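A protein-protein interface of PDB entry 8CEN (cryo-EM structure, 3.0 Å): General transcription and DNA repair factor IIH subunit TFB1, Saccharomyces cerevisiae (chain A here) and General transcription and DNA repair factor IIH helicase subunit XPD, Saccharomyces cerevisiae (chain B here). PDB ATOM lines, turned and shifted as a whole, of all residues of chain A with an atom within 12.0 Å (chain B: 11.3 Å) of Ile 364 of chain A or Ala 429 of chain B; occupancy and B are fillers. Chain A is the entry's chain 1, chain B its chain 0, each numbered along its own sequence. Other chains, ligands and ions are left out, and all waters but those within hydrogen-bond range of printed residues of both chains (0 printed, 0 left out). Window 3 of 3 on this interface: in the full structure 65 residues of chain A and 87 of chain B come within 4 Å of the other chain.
The side-chain amide nitrogen (ND2) of Asn 427 of chain B lies within hydrogen-bond range of the backbone carbonyl oxygen (O) of Val 362 of chain A, at 2.5 Å. The backbone NH (N) of Ala 429 of chain B is in hydrogen-bond range of the backbone carbonyl oxygen (O) of Ile 364 of chain A (2.7 Å).
The side-chain carboxylate (OD2) of Asp 363 of chain A is in hydrogen-bond range of the side-chain amide nitrogen (ND2) of Asn 367 of chain A.
Ile 425 of chain B touches Val 362 of chain A (CD1 to CG2, 3.7 Å). Asp 363 of chain A touches Asn 427 of chain B. O of Asn 427 of chain B touches CD1 of Ile 364 of chain A, at 3.4 Å. CA of Ala 428 of chain B touches O of Ile 364 of chain A, at 3.3 Å.
Of the printed residues of chain B, Val 362 of chain A touches Ile 425 and Asn 427. Ile 364 of chain A touches just these residues of chain B: Asn 427 (3.4 Å), Ala 428 (3.3 Å) and Ala 429 (2.7 Å). No residue of chain B comes within 4 Å of Asn 365 of chain A. Gly 366 of chain A touches none of the printed residues of chain B. No residue of chain B comes within 4 Å of Asn 367 of chain A. Ser 368 of chain A touches none of the printed residues of chain B. Glu 424 of chain B touches none of the printed residues of chain A. Of the printed residues of chain A, Ile 425 of chain B touches Val 362. Of chain A, only Val 362 (2.5 Å), Asp 363 (3.6 Å) and Ile 364 (3.4 Å) come within 4 Å of Asn 427 of chain B. Ala 428 of chain B touches just one residue of chain A: Ile 364 (3.3 Å). Ala 429 of chain B touches just one residue of chain A: Ile 364 (2.7 Å). No residue of chain A comes within 4 Å of Val 430 of chain B. No residue of chain A comes within 4 Å of Pro 431 of chain B. The nearest residue of chain B that does not touch Ile 364 of chain A is Val 430 of chain B (5.0 Å). The nearest residue of chain A that does not touch Ala 429 of chain B is Asn 365 of chain A (4.8 Å).
Of the 14 printed residues of chain A, 3 touch a printed residue of chain B. Hydrophobic or aromatic side chains of chain A that line the printed part of chain B: Val 362 and Ile 364. Hydrophobic or aromatic side chains of chain B within 4 Å of the printed part of chain A: Ile 425 and Ala 429. Along chain B the printed residues that touch a printed residue of chain A span positions 425 to 429. Among the printed residues, no Asp or Glu carboxylate lies within 4 Å of a Lys or Arg side-chain nitrogen of the other chain.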
ATOM      1  N   LYS A 300      29.198  14.369  36.631  1.00  0.00           N
ATOM      2  CA  LYS A 300      28.756  13.526  35.525  1.00  0.00           C
ATOM      3  C   LYS A 300      27.535  14.142  34.853  1.00  0.00           C
ATOM      4  O   LYS A 300      26.530  14.420  35.511  1.00  0.00           O
ATOM      5  CB  LYS A 300      28.438  12.120  36.027  1.00  0.00           C
ATOM      6  CG  LYS A 300      29.658  11.295  36.394  1.00  0.00           C
ATOM      7  CD  LYS A 300      29.282   9.843  36.636  1.00  0.00           C
ATOM      8  CE  LYS A 300      28.681   9.216  35.388  1.00  0.00           C
ATOM      9  NZ  LYS A 300      28.266   7.805  35.621  1.00  0.00           N
ATOM     10  N   PHE A 356      35.598  -7.551  34.025  1.00  0.00           N
ATOM     11  CA  PHE A 356      34.956  -6.249  33.849  1.00  0.00           C
ATOM     12  C   PHE A 356      35.330  -5.230  34.918  1.00  0.00           C
ATOM     13  O   PHE A 356      35.080  -4.036  34.719  1.00  0.00           O
ATOM     14  CB  PHE A 356      33.434  -6.418  33.808  1.00  0.00           C
ATOM     15  CG  PHE A 356      32.797  -6.575  35.165  1.00  0.00           C
ATOM     16  CD1 PHE A 356      33.048  -7.695  35.943  1.00  0.00           C
ATOM     17  CD2 PHE A 356      31.941  -5.603  35.655  1.00  0.00           C
ATOM     18  CE1 PHE A 356      32.463  -7.839  37.186  1.00  0.00           C
ATOM     19  CE2 PHE A 356      31.351  -5.743  36.899  1.00  0.00           C
ATOM     20  CZ  PHE A 356      31.614  -6.862  37.663  1.00  0.00           C
ATOM     21  N   PRO A 360      36.900   0.260  32.015  1.00  0.00           N
ATOM     22  CA  PRO A 360      35.921   1.279  32.412  1.00  0.00           C
ATOM     23  C   PRO A 360      34.497   0.747  32.376  1.00  0.00           C
ATOM     24  O   PRO A 360      34.161  -0.141  31.589  1.00  0.00           O
ATOM     25  CB  PRO A 360      36.126   2.392  31.378  1.00  0.00           C
ATOM     26  CG  PRO A 360      37.528   2.243  30.943  1.00  0.00           C
ATOM     27  CD  PRO A 360      37.839   0.778  30.998  1.00  0.00           C
ATOM     28  N   GLY A 361      33.667   1.292  33.262  1.00  0.00           N
ATOM     29  CA  GLY A 361      32.295   0.838  33.366  1.00  0.00           C
ATOM     30  C   GLY A 361      31.485   1.161  32.124  1.00  0.00           C
ATOM     31  O   GLY A 361      31.738   2.136  31.416  1.00  0.00           O
ATOM     32  N   VAL A 362      30.493   0.313  31.860  1.00  0.00           N
ATOM     33  CA  VAL A 362      29.690   0.403  30.651  1.00  0.00           C
ATOM     34  C   VAL A 362      28.216   0.433  31.031  1.00  0.00           C
ATOM     35  O   VAL A 362      27.820   0.022  32.124  1.00  0.00           O
ATOM     36  CB  VAL A 362      29.969  -0.764  29.680  1.00  0.00           C
ATOM     37  CG1 VAL A 362      31.332  -0.597  29.027  1.00  0.00           C
ATOM     38  CG2 VAL A 362      29.887  -2.090  30.417  1.00  0.00           C
ATOM     39  N   ASP A 363      27.405   0.932  30.104  1.00  0.00           N
ATOM     40  CA  ASP A 363      25.964   1.007  30.295  1.00  0.00           C
ATOM     41  C   ASP A 363      25.332  -0.348  29.973  1.00  0.00           C
ATOM     42  O   ASP A 363      26.015  -1.362  29.814  1.00  0.00           O
ATOM     43  CB  ASP A 363      25.375   2.126  29.441  1.00  0.00           C
ATOM     44  CG  ASP A 363      25.784   3.503  29.922  1.00  0.00           C
ATOM     45  OD1 ASP A 363      26.022   3.662  31.137  1.00  0.00           O
ATOM     46  OD2 ASP A 363      25.868   4.426  29.085  1.00  0.00           O
ATOM     47  N   ILE A 364      24.000  -0.372  29.886  1.00  0.00           N
ATOM     48  CA  ILE A 364      23.299  -1.598  29.520  1.00  0.00           C
ATOM     49  C   ILE A 364      23.561  -1.952  28.058  1.00  0.00           C
ATOM     50  O   ILE A 364      23.629  -3.134  27.698  1.00  0.00           O
ATOM     51  CB  ILE A 364      21.794  -1.451  29.843  1.00  0.00           C
ATOM     52  CG1 ILE A 364      21.015  -2.721  29.487  1.00  0.00           C
ATOM     53  CG2 ILE A 364      21.197  -0.220  29.164  1.00  0.00           C
ATOM     54  CD1 ILE A 364      21.224  -3.859  30.463  1.00  0.00           C
ATOM     55  N   ASN A 365      23.755  -0.949  27.202  1.00  0.00           N
ATOM     56  CA  ASN A 365      24.034  -1.165  25.789  1.00  0.00           C
ATOM     57  C   ASN A 365      25.516  -1.380  25.500  1.00  0.00           C
ATOM     58  O   ASN A 365      25.878  -1.606  24.341  1.00  0.00           O
ATOM     59  CB  ASN A 365      23.519   0.019  24.965  1.00  0.00           C
ATOM     60  CG  ASN A 365      22.021   0.206  25.089  1.00  0.00           C
ATOM     61  OD1 ASN A 365      21.550   1.218  25.610  1.00  0.00           O
ATOM     62  ND2 ASN A 365      21.261  -0.772  24.610  1.00  0.00           N
ATOM     63  N   GLY A 366      26.375  -1.317  26.516  1.00  0.00           N
ATOM     64  CA  GLY A 366      27.796  -1.518  26.339  1.00  0.00           C
ATOM     65  C   GLY A 366      28.599  -0.264  26.065  1.00  0.00           C
ATOM     66  O   GLY A 366      29.833  -0.336  26.029  1.00  0.00           O
ATOM     67  N   ASN A 367      27.946   0.879  25.868  1.00  0.00           N
ATOM     68  CA  ASN A 367      28.655   2.129  25.660  1.00  0.00           C
ATOM     69  C   ASN A 367      29.215   2.653  26.980  1.00  0.00           C
ATOM     70  O   ASN A 367      28.813   2.229  28.066  1.00  0.00           O
ATOM     71  CB  ASN A 367      27.733   3.172  25.026  1.00  0.00           C
ATOM     72  CG  ASN A 367      26.497   3.439  25.861  1.00  0.00           C
ATOM     73  OD1 ASN A 367      25.565   2.636  25.885  1.00  0.00           O
ATOM     74  ND2 ASN A 367      26.483   4.574  26.551  1.00  0.00           N
ATOM     75  N   SER A 368      30.157   3.588  26.870  1.00  0.00           N
ATOM     76  CA  SER A 368      30.810   4.145  28.048  1.00  0.00           C
ATOM     77  C   SER A 368      29.839   4.991  28.863  1.00  0.00           C
ATOM     78  O   SER A 368      29.004   5.714  28.312  1.00  0.00           O
ATOM     79  CB  SER A 368      32.017   4.987  27.635  1.00  0.00           C
ATOM     80  OG  SER A 368      31.612   6.252  27.145  1.00  0.00           O
ATOM     81  N   ASP A 369      29.953   4.894  30.185  1.00  0.00           N
ATOM     82  CA  ASP A 369      29.067   5.600  31.102  1.00  0.00           C
ATOM     83  C   ASP A 369      29.525   7.018  31.427  1.00  0.00           C
ATOM     84  O   ASP A 369      28.819   7.731  32.147  1.00  0.00           O
ATOM     85  CB  ASP A 369      28.883   4.782  32.392  1.00  0.00           C
ATOM     86  CG  ASP A 369      30.199   4.469  33.110  1.00  0.00           C
ATOM     87  OD1 ASP A 369      31.258   5.045  32.785  1.00  0.00           O
ATOM     88  OD2 ASP A 369      30.164   3.620  34.028  1.00  0.00           O
ATOM     89  N   GLY A 370      30.682   7.442  30.921  1.00  0.00           N
ATOM     90  CA  GLY A 370      31.184   8.773  31.179  1.00  0.00           C
ATOM     91  C   GLY A 370      31.978   8.931  32.457  1.00  0.00           C
ATOM     92  O   GLY A 370      32.401  10.052  32.766  1.00  0.00           O
ATOM     93  N   THR A 371      32.182   7.852  33.216  1.00  0.00           N
ATOM     94  CA  THR A 371      32.992   7.941  34.428  1.00  0.00           C
ATOM     95  C   THR A 371      34.458   8.189  34.097  1.00  0.00           C
ATOM     96  O   THR A 371      35.151   8.910  34.824  1.00  0.00           O
ATOM     97  CB  THR A 371      32.840   6.670  35.262  1.00  0.00           C
ATOM     98  OG1 THR A 371      33.007   5.521  34.422  1.00  0.00           O
ATOM     99  CG2 THR A 371      31.467   6.621  35.917  1.00  0.00           C
ATOM    100  N   PRO B 422      28.589 -17.578  27.838  1.00  0.00           N
ATOM    101  CA  PRO B 422      27.583 -16.888  27.013  1.00  0.00           C
ATOM    102  C   PRO B 422      27.605 -15.379  27.171  1.00  0.00           C
ATOM    103  O   PRO B 422      27.278 -14.659  26.219  1.00  0.00           O
ATOM    104  CB  PRO B 422      26.260 -17.491  27.504  1.00  0.00           C
ATOM    105  CG  PRO B 422      26.546 -17.931  28.899  1.00  0.00           C
ATOM    106  CD  PRO B 422      27.975 -18.393  28.900  1.00  0.00           C
ATOM    107  N   TYR B 423      27.979 -14.878  28.345  1.00  0.00           N
ATOM    108  CA  TYR B 423      28.059 -13.446  28.614  1.00  0.00           C
ATOM    109  C   TYR B 423      29.509 -13.096  28.920  1.00  0.00           C
ATOM    110  O   TYR B 423      30.058 -13.547  29.932  1.00  0.00           O
ATOM    111  CB  TYR B 423      27.150 -13.056  29.778  1.00  0.00           C
ATOM    112  CG  TYR B 423      25.723 -12.756  29.382  1.00  0.00           C
ATOM    113  CD1 TYR B 423      24.765 -13.762  29.343  1.00  0.00           C
ATOM    114  CD2 TYR B 423      25.331 -11.463  29.056  1.00  0.00           C
ATOM    115  CE1 TYR B 423      23.458 -13.491  28.984  1.00  0.00           C
ATOM    116  CE2 TYR B 423      24.025 -11.182  28.696  1.00  0.00           C
ATOM    117  CZ  TYR B 423      23.093 -12.200  28.663  1.00  0.00           C
ATOM    118  OH  TYR B 423      21.793 -11.925  28.305  1.00  0.00           O
ATOM    119  N   GLU B 424      30.133 -12.310  28.041  1.00  0.00           N
ATOM    120  CA  GLU B 424      31.453 -11.768  28.344  1.00  0.00           C
ATOM    121  C   GLU B 424      31.382 -10.806  29.522  1.00  0.00           C
ATOM    122  O   GLU B 424      32.206 -10.863  30.442  1.00  0.00           O
ATOM    123  CB  GLU B 424      32.032 -11.069  27.113  1.00  0.00           C
ATOM    124  CG  GLU B 424      33.440 -10.538  27.304  1.00  0.00           C
ATOM    125  CD  GLU B 424      33.994  -9.899  26.047  1.00  0.00           C
ATOM    126  OE1 GLU B 424      33.268  -9.852  25.033  1.00  0.00           O
ATOM    127  OE2 GLU B 424      35.154  -9.441  26.075  1.00  0.00           O
ATOM    128  N   ILE B 425      30.395  -9.914  29.507  1.00  0.00           N
ATOM    129  CA  ILE B 425      30.091  -9.031  30.626  1.00  0.00           C
ATOM    130  C   ILE B 425      28.603  -9.149  30.932  1.00  0.00           C
ATOM    131  O   ILE B 425      27.779  -9.298  30.023  1.00  0.00           O
ATOM    132  CB  ILE B 425      30.499  -7.566  30.340  1.00  0.00           C
ATOM    133  CG1 ILE B 425      29.772  -7.010  29.112  1.00  0.00           C
ATOM    134  CG2 ILE B 425      32.010  -7.438  30.182  1.00  0.00           C
ATOM    135  CD1 ILE B 425      29.952  -5.523  28.915  1.00  0.00           C
ATOM    136  N   GLU B 426      28.265  -9.135  32.222  1.00  0.00           N
ATOM    137  CA  GLU B 426      26.871  -9.265  32.627  1.00  0.00           C
ATOM    138  C   GLU B 426      26.099  -7.959  32.512  1.00  0.00           C
ATOM    139  O   GLU B 426      24.864  -7.979  32.542  1.00  0.00           O
ATOM    140  CB  GLU B 426      26.787  -9.790  34.062  1.00  0.00           C
ATOM    141  CG  GLU B 426      27.779 -10.900  34.369  1.00  0.00           C
ATOM    142  CD  GLU B 426      27.575 -12.121  33.493  1.00  0.00           C
ATOM    143  OE1 GLU B 426      26.409 -12.516  33.280  1.00  0.00           O
ATOM    144  OE2 GLU B 426      28.582 -12.684  33.014  1.00  0.00           O
ATOM    145  N   ASN B 427      26.796  -6.829  32.380  1.00  0.00           N
ATOM    146  CA  ASN B 427      26.121  -5.540  32.274  1.00  0.00           C
ATOM    147  C   ASN B 427      25.490  -5.327  30.904  1.00  0.00           C
ATOM    148  O   ASN B 427      24.540  -4.546  30.789  1.00  0.00           O
ATOM    149  CB  ASN B 427      27.106  -4.410  32.580  1.00  0.00           C
ATOM    150  CG  ASN B 427      26.415  -3.137  33.030  1.00  0.00           C
ATOM    151  OD1 ASN B 427      25.198  -3.103  33.203  1.00  0.00           O
ATOM    152  ND2 ASN B 427      27.195  -2.079  33.221  1.00  0.00           N
ATOM    153  N   ALA B 428      25.995  -5.995  29.870  1.00  0.00           N
ATOM    154  CA  ALA B 428      25.486  -5.788  28.521  1.00  0.00           C
ATOM    155  C   ALA B 428      24.109  -6.417  28.352  1.00  0.00           C
ATOM    156  O   ALA B 428      23.813  -7.470  28.923  1.00  0.00           O
ATOM    157  CB  ALA B 428      26.455  -6.370  27.493  1.00  0.00           C
ATOM    158  N   ALA B 429      23.262  -5.757  27.560  1.00  0.00           N
ATOM    159  CA  ALA B 429      21.928  -6.282  27.289  1.00  0.00           C
ATOM    160  C   ALA B 429      21.990  -7.469  26.337  1.00  0.00           C
ATOM    161  O   ALA B 429      21.559  -8.578  26.673  1.00  0.00           O
ATOM    162  CB  ALA B 429      21.035  -5.179  26.719  1.00  0.00           C
ATOM    163  N   VAL B 430      22.518  -7.252  25.139  1.00  0.00           N
ATOM    164  CA  VAL B 430      22.679  -8.347  24.176  1.00  0.00           C
ATOM    165  C   VAL B 430      23.806  -9.266  24.646  1.00  0.00           C
ATOM    166  O   VAL B 430      24.841  -8.775  25.136  1.00  0.00           O
ATOM    167  CB  VAL B 430      22.940  -7.787  22.765  1.00  0.00           C
ATOM    168  CG1 VAL B 430      24.141  -6.839  22.735  1.00  0.00           C
ATOM    169  CG2 VAL B 430      23.114  -8.910  21.749  1.00  0.00           C
ATOM    170  N   PRO B 431      23.624 -10.587  24.609  1.00  0.00           N
ATOM    171  CA  PRO B 431      24.710 -11.487  25.016  1.00  0.00           C
ATOM    172  C   PRO B 431      25.887 -11.421  24.056  1.00  0.00           C
ATOM    173  O   PRO B 431      25.719 -11.329  22.837  1.00  0.00           O
ATOM    174  CB  PRO B 431      24.051 -12.871  24.992  1.00  0.00           C
ATOM    175  CG  PRO B 431      22.595 -12.600  25.145  1.00  0.00           C
ATOM    176  CD  PRO B 431      22.350 -11.304  24.432  1.00  0.00           C
ATOM    177  N   ASN B 432      27.090 -11.471  24.623  1.00  0.00           N
ATOM    178  CA  ASN B 432      28.331 -11.521  23.854  1.00  0.00           C
ATOM    179  C   ASN B 432      29.121 -12.737  24.315  1.00  0.00           C
ATOM    180  O   ASN B 432      29.765 -12.691  25.378  1.00  0.00           O
ATOM    181  CB  ASN B 432      29.148 -10.246  24.017  1.00  0.00           C
ATOM    182  CG  ASN B 432      28.505  -9.052  23.341  1.00  0.00           C
ATOM    183  OD1 ASN B 432      27.989  -9.158  22.229  1.00  0.00           O
ATOM    184  ND2 ASN B 432      28.536  -7.905  24.009  1.00  0.00           N
ATOM    185  N   PRO B 433      29.074 -13.840  23.573  1.00  0.00           N
ATOM    186  CA  PRO B 433      29.830 -15.031  23.975  1.00  0.00           C
ATOM    187  C   PRO B 433      31.328 -14.807  23.862  1.00  0.00           C
ATOM    188  O   PRO B 433      31.803 -13.978  23.081  1.00  0.00           O
ATOM    189  CB  PRO B 433      29.354 -16.109  22.990  1.00  0.00           C
ATOM    190  CG  PRO B 433      28.122 -15.546  22.340  1.00  0.00           C
ATOM    191  CD  PRO B 433      28.304 -14.066  22.341  1.00  0.00           C
